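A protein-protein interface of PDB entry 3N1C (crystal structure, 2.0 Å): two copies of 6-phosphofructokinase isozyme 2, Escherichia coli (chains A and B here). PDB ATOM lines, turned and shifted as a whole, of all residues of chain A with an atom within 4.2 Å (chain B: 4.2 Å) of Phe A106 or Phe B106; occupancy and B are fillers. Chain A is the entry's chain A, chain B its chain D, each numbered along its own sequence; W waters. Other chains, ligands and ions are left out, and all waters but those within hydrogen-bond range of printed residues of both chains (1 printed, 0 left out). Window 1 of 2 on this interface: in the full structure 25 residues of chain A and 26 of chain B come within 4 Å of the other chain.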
ATOM      1  N   LEU A  28      18.706 -19.626 -23.332  1.00  0.00           N
ATOM      2  CA  LEU A  28      17.817 -19.143 -24.378  1.00  0.00           C
ATOM      3  C   LEU A  28      18.590 -18.268 -25.362  1.00  0.00           C
ATOM      4  O   LEU A  28      19.005 -17.159 -25.027  1.00  0.00           O
ATOM      5  CB  LEU A  28      16.641 -18.377 -23.769  1.00  0.00           C
ATOM      6  CG  LEU A  28      15.866 -19.134 -22.682  1.00  0.00           C
ATOM      7  CD1 LEU A  28      14.717 -18.287 -22.140  1.00  0.00           C
ATOM      8  CD2 LEU A  28      15.349 -20.466 -23.208  1.00  0.00           C
ATOM      9  N   CYS A  30      19.317 -15.688 -27.822  1.00  0.00           N
ATOM     10  CA  CYS A  30      18.666 -14.451 -28.247  1.00  0.00           C
ATOM     11  C   CYS A  30      19.453 -13.742 -29.335  1.00  0.00           C
ATOM     12  O   CYS A  30      20.669 -13.895 -29.437  1.00  0.00           O
ATOM     13  CB  CYS A  30      18.470 -13.502 -27.062  1.00  0.00           C
ATOM     14  SG  CYS A  30      17.459 -14.171 -25.729  1.00  0.00           S
ATOM     15  N   ASN A  92      16.464  -1.753 -20.046  1.00  0.00           N
ATOM     16  CA  ASN A  92      15.424  -2.758 -19.878  1.00  0.00           C
ATOM     17  C   ASN A  92      15.432  -3.754 -21.031  1.00  0.00           C
ATOM     18  O   ASN A  92      15.923  -3.451 -22.117  1.00  0.00           O
ATOM     19  CB  ASN A  92      14.059  -2.085 -19.726  1.00  0.00           C
ATOM     20  CG  ASN A  92      13.948  -1.298 -18.429  1.00  0.00           C
ATOM     21  OD1 ASN A  92      14.735  -1.505 -17.506  1.00  0.00           O
ATOM     22  ND2 ASN A  92      12.962  -0.402 -18.347  1.00  0.00           N
ATOM     23  N   LEU A  93      14.908  -4.950 -20.794  1.00  0.00           N
ATOM     24  CA  LEU A  93      14.944  -5.985 -21.815  1.00  0.00           C
ATOM     25  C   LEU A  93      13.551  -6.422 -22.232  1.00  0.00           C
ATOM     26  O   LEU A  93      12.737  -6.816 -21.399  1.00  0.00           O
ATOM     27  CB  LEU A  93      15.753  -7.195 -21.339  1.00  0.00           C
ATOM     28  CG  LEU A  93      15.878  -8.312 -22.381  1.00  0.00           C
ATOM     29  CD1 LEU A  93      16.566  -7.807 -23.642  1.00  0.00           C
ATOM     30  CD2 LEU A  93      16.615  -9.509 -21.811  1.00  0.00           C
ATOM     31  N   VAL A  95      11.654  -9.182 -24.555  1.00  0.00           N
ATOM     32  CA  VAL A  95      11.904 -10.447 -25.231  1.00  0.00           C
ATOM     33  C   VAL A  95      10.674 -10.981 -25.964  1.00  0.00           C
ATOM     34  O   VAL A  95       9.621 -11.201 -25.360  1.00  0.00           O
ATOM     35  CB  VAL A  95      12.404 -11.516 -24.240  1.00  0.00           C
ATOM     36  CG1 VAL A  95      12.809 -12.775 -24.983  1.00  0.00           C
ATOM     37  CG2 VAL A  95      13.573 -10.970 -23.419  1.00  0.00           C
ATOM     38  N   TYR A 104       7.920 -10.659 -23.322  1.00  0.00           N
ATOM     39  CA  TYR A 104       8.271 -10.518 -21.914  1.00  0.00           C
ATOM     40  C   TYR A 104       9.062  -9.246 -21.663  1.00  0.00           C
ATOM     41  O   TYR A 104       9.970  -8.904 -22.424  1.00  0.00           O
ATOM     42  CB  TYR A 104       9.036 -11.747 -21.431  1.00  0.00           C
ATOM     43  CG  TYR A 104       8.178 -12.987 -21.411  1.00  0.00           C
ATOM     44  CD1 TYR A 104       8.078 -13.802 -22.531  1.00  0.00           C
ATOM     45  CD2 TYR A 104       7.452 -13.331 -20.281  1.00  0.00           C
ATOM     46  CE1 TYR A 104       7.279 -14.933 -22.524  1.00  0.00           C
ATOM     47  CE2 TYR A 104       6.650 -14.461 -20.262  1.00  0.00           C
ATOM     48  CZ  TYR A 104       6.567 -15.259 -21.384  1.00  0.00           C
ATOM     49  OH  TYR A 104       5.772 -16.386 -21.362  1.00  0.00           O
ATOM     50  N   ARG A 105       8.714  -8.550 -20.587  1.00  0.00           N
ATOM     51  CA  ARG A 105       9.260  -7.223 -20.340  1.00  0.00           C
ATOM     52  C   ARG A 105       9.944  -7.137 -18.984  1.00  0.00           C
ATOM     53  O   ARG A 105       9.289  -7.152 -17.942  1.00  0.00           O
ATOM     54  CB  ARG A 105       8.147  -6.178 -20.448  1.00  0.00           C
ATOM     55  CG  ARG A 105       7.419  -6.234 -21.783  1.00  0.00           C
ATOM     56  CD  ARG A 105       6.101  -5.502 -21.719  1.00  0.00           C
ATOM     57  NE  ARG A 105       6.288  -4.065 -21.587  1.00  0.00           N
ATOM     58  CZ  ARG A 105       5.380  -3.249 -21.067  1.00  0.00           C
ATOM     59  NH1 ARG A 105       4.228  -3.739 -20.626  1.00  0.00           N
ATOM     60  NH2 ARG A 105       5.624  -1.948 -20.984  1.00  0.00           N
ATOM     61  N   PHE A 106      11.268  -7.037 -19.010  1.00  0.00           N
ATOM     62  CA  PHE A 106      12.053  -6.970 -17.787  1.00  0.00           C
ATOM     63  C   PHE A 106      12.482  -5.535 -17.499  1.00  0.00           C
ATOM     64  O   PHE A 106      13.297  -4.945 -18.211  1.00  0.00           O
ATOM     65  CB  PHE A 106      13.240  -7.929 -17.868  1.00  0.00           C
ATOM     66  CG  PHE A 106      12.829  -9.357 -18.101  1.00  0.00           C
ATOM     67  CD1 PHE A 106      12.867  -9.907 -19.370  1.00  0.00           C
ATOM     68  CD2 PHE A 106      12.372 -10.137 -17.048  1.00  0.00           C
ATOM     69  CE1 PHE A 106      12.471 -11.211 -19.580  1.00  0.00           C
ATOM     70  CE2 PHE A 106      11.973 -11.435 -17.254  1.00  0.00           C
ATOM     71  CZ  PHE A 106      12.028 -11.977 -18.520  1.00  0.00           C
ATOM     72  N   VAL A 107      11.902  -4.982 -16.445  1.00  0.00           N
ATOM     73  CA  VAL A 107      12.021  -3.567 -16.153  1.00  0.00           C
ATOM     74  C   VAL A 107      12.870  -3.359 -14.905  1.00  0.00           C
ATOM     75  O   VAL A 107      12.427  -3.644 -13.793  1.00  0.00           O
ATOM     76  CB  VAL A 107      10.618  -2.965 -15.940  1.00  0.00           C
ATOM     77  CG1 VAL A 107      10.704  -1.489 -15.591  1.00  0.00           C
ATOM     78  CG2 VAL A 107       9.745  -3.205 -17.180  1.00  0.00           C
ATOM     79  N   MET A 108      14.054  -2.780 -15.220  1.00  0.00           N
ATOM     80  CA  MET A 108      15.063  -2.629 -14.176  1.00  0.00           C
ATOM     81  C   MET A 108      14.760  -1.400 -13.316  1.00  0.00           C
ATOM     82  O   MET A 108      13.921  -0.571 -13.677  1.00  0.00           O
ATOM     83  CB  MET A 108      16.464  -2.480 -14.790  1.00  0.00           C
ATOM     84  CG  MET A 108      16.977  -3.679 -15.567  1.00  0.00           C
ATOM     85  SD  MET A 108      17.190  -5.173 -14.578  1.00  0.00           S
ATOM     86  CE  MET A 108      15.750  -6.099 -15.068  1.00  0.00           C
ATOM     87  N   LEU B  28       7.514  -6.616 -15.735  1.00  0.00           N
ATOM     88  CA  LEU B  28       8.059  -7.405 -14.642  1.00  0.00           C
ATOM     89  C   LEU B  28       9.147  -6.607 -13.926  1.00  0.00           C
ATOM     90  O   LEU B  28      10.233  -6.380 -14.471  1.00  0.00           O
ATOM     91  CB  LEU B  28       8.596  -8.738 -15.163  1.00  0.00           C
ATOM     92  CG  LEU B  28       7.623  -9.493 -16.074  1.00  0.00           C
ATOM     93  CD1 LEU B  28       8.288 -10.707 -16.717  1.00  0.00           C
ATOM     94  CD2 LEU B  28       6.366  -9.901 -15.306  1.00  0.00           C
ATOM     95  N   CYS B  30      12.112  -5.777 -11.915  1.00  0.00           N
ATOM     96  CA  CYS B  30      13.337  -6.483 -11.554  1.00  0.00           C
ATOM     97  C   CYS B  30      14.205  -5.658 -10.611  1.00  0.00           C
ATOM     98  O   CYS B  30      14.201  -4.426 -10.658  1.00  0.00           O
ATOM     99  CB  CYS B  30      14.129  -6.854 -12.811  1.00  0.00           C
ATOM    100  SG  CYS B  30      13.285  -7.998 -13.928  1.00  0.00           S
ATOM    101  N   ASN B  92      24.562 -10.658 -20.922  1.00  0.00           N
ATOM    102  CA  ASN B  92      23.490 -11.636 -20.824  1.00  0.00           C
ATOM    103  C   ASN B  92      22.707 -11.407 -19.533  1.00  0.00           C
ATOM    104  O   ASN B  92      23.291 -11.092 -18.495  1.00  0.00           O
ATOM    105  CB  ASN B  92      24.060 -13.052 -20.886  1.00  0.00           C
ATOM    106  CG  ASN B  92      24.699 -13.370 -22.234  1.00  0.00           C
ATOM    107  OD1 ASN B  92      24.485 -12.662 -23.219  1.00  0.00           O
ATOM    108  ND2 ASN B  92      25.485 -14.442 -22.280  1.00  0.00           N
ATOM    109  N   LEU B  93      21.387 -11.548 -19.601  1.00  0.00           N
ATOM    110  CA  LEU B  93      20.533 -11.309 -18.440  1.00  0.00           C
ATOM    111  C   LEU B  93      20.047 -12.614 -17.818  1.00  0.00           C
ATOM    112  O   LEU B  93      19.500 -13.481 -18.506  1.00  0.00           O
ATOM    113  CB  LEU B  93      19.327 -10.443 -18.816  1.00  0.00           C
ATOM    114  CG  LEU B  93      18.409 -10.033 -17.657  1.00  0.00           C
ATOM    115  CD1 LEU B  93      19.105  -9.040 -16.721  1.00  0.00           C
ATOM    116  CD2 LEU B  93      17.106  -9.447 -18.183  1.00  0.00           C
ATOM    117  N   VAL B  95      17.506 -14.034 -14.928  1.00  0.00           N
ATOM    118  CA  VAL B  95      16.382 -13.596 -14.119  1.00  0.00           C
ATOM    119  C   VAL B  95      15.961 -14.714 -13.190  1.00  0.00           C
ATOM    120  O   VAL B  95      15.511 -15.761 -13.643  1.00  0.00           O
ATOM    121  CB  VAL B  95      15.174 -13.210 -14.979  1.00  0.00           C
ATOM    122  CG1 VAL B  95      14.063 -12.641 -14.102  1.00  0.00           C
ATOM    123  CG2 VAL B  95      15.573 -12.214 -16.063  1.00  0.00           C
ATOM    124  N   TYR B 104      15.790 -17.841 -15.454  1.00  0.00           N
ATOM    125  CA  TYR B 104      15.735 -17.736 -16.910  1.00  0.00           C
ATOM    126  C   TYR B 104      16.991 -17.062 -17.434  1.00  0.00           C
ATOM    127  O   TYR B 104      17.478 -16.101 -16.842  1.00  0.00           O
ATOM    128  CB  TYR B 104      14.484 -16.972 -17.348  1.00  0.00           C
ATOM    129  CG  TYR B 104      13.207 -17.745 -17.107  1.00  0.00           C
ATOM    130  CD1 TYR B 104      12.662 -17.841 -15.831  1.00  0.00           C
ATOM    131  CD2 TYR B 104      12.554 -18.393 -18.152  1.00  0.00           C
ATOM    132  CE1 TYR B 104      11.503 -18.553 -15.604  1.00  0.00           C
ATOM    133  CE2 TYR B 104      11.391 -19.108 -17.933  1.00  0.00           C
ATOM    134  CZ  TYR B 104      10.870 -19.183 -16.656  1.00  0.00           C
ATOM    135  OH  TYR B 104       9.712 -19.891 -16.428  1.00  0.00           O
ATOM    136  N   ARG B 105      17.523 -17.575 -18.539  1.00  0.00           N
ATOM    137  CA  ARG B 105      18.800 -17.095 -19.052  1.00  0.00           C
ATOM    138  C   ARG B 105      18.681 -16.610 -20.482  1.00  0.00           C
ATOM    139  O   ARG B 105      18.453 -17.398 -21.402  1.00  0.00           O
ATOM    140  CB  ARG B 105      19.858 -18.193 -18.959  1.00  0.00           C
ATOM    141  CG  ARG B 105      20.015 -18.770 -17.563  1.00  0.00           C
ATOM    142  CD  ARG B 105      20.540 -20.189 -17.628  1.00  0.00           C
ATOM    143  NE  ARG B 105      21.989 -20.244 -17.772  1.00  0.00           N
ATOM    144  CZ  ARG B 105      22.664 -21.344 -18.082  1.00  0.00           C
ATOM    145  NH1 ARG B 105      22.021 -22.484 -18.296  1.00  0.00           N
ATOM    146  NH2 ARG B 105      23.984 -21.304 -18.181  1.00  0.00           N
ATOM    147  N   PHE B 106      18.841 -15.307 -20.662  1.00  0.00           N
ATOM    148  CA  PHE B 106      18.756 -14.715 -21.982  1.00  0.00           C
ATOM    149  C   PHE B 106      20.150 -14.440 -22.536  1.00  0.00           C
ATOM    150  O   PHE B 106      20.818 -13.476 -22.155  1.00  0.00           O
ATOM    151  CB  PHE B 106      17.872 -13.477 -21.931  1.00  0.00           C
ATOM    152  CG  PHE B 106      16.492 -13.767 -21.407  1.00  0.00           C
ATOM    153  CD1 PHE B 106      16.184 -13.554 -20.072  1.00  0.00           C
ATOM    154  CD2 PHE B 106      15.519 -14.302 -22.239  1.00  0.00           C
ATOM    155  CE1 PHE B 106      14.923 -13.838 -19.585  1.00  0.00           C
ATOM    156  CE2 PHE B 106      14.251 -14.588 -21.760  1.00  0.00           C
ATOM    157  CZ  PHE B 106      13.952 -14.352 -20.432  1.00  0.00           C
ATOM    158  N   VAL B 107      20.579 -15.324 -23.429  1.00  0.00           N
ATOM    159  CA  VAL B 107      21.952 -15.354 -23.901  1.00  0.00           C
ATOM    160  C   VAL B 107      22.080 -14.745 -25.292  1.00  0.00           C
ATOM    161  O   VAL B 107      21.689 -15.354 -26.290  1.00  0.00           O
ATOM    162  CB  VAL B 107      22.498 -16.791 -23.898  1.00  0.00           C
ATOM    163  CG1 VAL B 107      23.929 -16.833 -24.413  1.00  0.00           C
ATOM    164  CG2 VAL B 107      22.415 -17.391 -22.495  1.00  0.00           C
ATOM    165  N   MET B 108      22.637 -13.538 -25.340  1.00  0.00           N
ATOM    166  CA  MET B 108      22.855 -12.815 -26.588  1.00  0.00           C
ATOM    167  C   MET B 108      24.053 -13.398 -27.327  1.00  0.00           C
ATOM    168  O   MET B 108      24.784 -14.221 -26.776  1.00  0.00           O
ATOM    169  CB  MET B 108      23.108 -11.336 -26.292  1.00  0.00           C
ATOM    170  CG  MET B 108      22.268 -10.793 -25.161  1.00  0.00           C
ATOM    171  SD  MET B 108      20.511 -10.722 -25.557  1.00  0.00           S
ATOM    172  CE  MET B 108      20.312  -8.979 -25.900  1.00  0.00           C
HETATM  173  O   HOH W   1      12.090  -2.310 -10.942  1.00  0.00           O
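Phe A106 touches four residues of chain B. Phe B106 touches just these residues of chain A: Leu A28, Cys A30, Val A95 and Phe A106. Printed residues of chain A within 4 Å of Arg B105: Leu A28 (3.0 Å). Printed residues of chain A within 4 Å of Leu B93: Leu A93 (3.7 Å). Of the printed residues of chain B, Arg A105 touches Leu B28 (2.9 Å). Printed residues of chain A within 4 Å of Met B108: Cys A30 (3.7 Å). Asn A92 touches none of the printed residues of chain B. The nearest printed residue of chain A that does not touch Met B108 is Leu A93 (4.5 Å).
Leu A28 touches Phe B106, and with the chains exchanged Phe A106 touches Leu B28. Cys A30 touches Val B107, and with the chains exchanged Val A107 touches Cys B30. Leu B93 touches its own counterpart, Leu A93. Val A95 touches Phe B106, and with the chains exchanged Phe A106 touches Val B95. Positions printed for both chains: 28, 30, 92, 93, 95, 104, 105, 106, 107 and 108.
N of Leu A28 sits at hydrogen-bond distance from O of Arg B105, 3.0 Å away. O of Leu A28 is in hydrogen-bond range of N of Val B107 (2.9 Å). The backbone NH (N) of Cys A30 is in hydrogen-bond range of the backbone carbonyl oxygen (O) of Val B107 (2.8 Å). The backbone carbonyl oxygen of Arg A105 is in hydrogen-bond range of the backbone NH of Leu B28 (2.9 Å). O of Leu B28 is in hydrogen-bond range of N of Val A107, at 2.9 Å. N of Cys B30 sits at hydrogen-bond distance from O of Val A107, 2.9 Å away.
Printed residues of chain B that touch a printed residue of chain A: Leu B28, Cys B30, Leu B93, Val B95, Arg B105, Phe B106, Val B107 and Met B108. Among the printed residues, no Asp or Glu carboxylate lies within 4 Å of a Lys or Arg side-chain nitrogen of the other chain.
Among the printed residues, merely in contact across the chains: Leu A28 with Phe B106 (3.7 Å), Cys A30 with Phe B106 (3.9 Å), Cys A30 with Met B108 (3.7 Å), Leu A93 with Leu B93 (3.7 Å), Val A95 with Phe B106 (3.97 Å), Phe A106 with Leu B28 (3.8 Å), Phe A106 with Cys B30 (3.9 Å), Phe A106 with Val B95 (3.9 Å), Phe A106 with Phe B106 (3.6 Å) and Met A108 with Cys B30 (2.9 Å).
Water W1 bridges O of Cys B30 (3.0 Å) and O of Val A107 (3.2 Å).
SG of Cys A30 is in hydrogen-bond range of O of Leu A28, at 3.4 Å. The backbone NH (N) of Met A108 lies within hydrogen-bond range of the side-chain amide oxygen (OD1) of Asn A92, 2.7 Å away. The backbone carbonyl oxygen (O) of Val A95 lies within hydrogen-bond range of the backbone NH (N) of Tyr A104. The backbone NH (N) of Met B108 lies within hydrogen-bond range of the side-chain amide oxygen (OD1) of Asn B92 (2.9 Å). N of Phe B106 sits at hydrogen-bond distance from O of Leu B93 (2.9 Å). O of Val B95 lies within hydrogen-bond range of N of Tyr B104 (2.8 Å).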
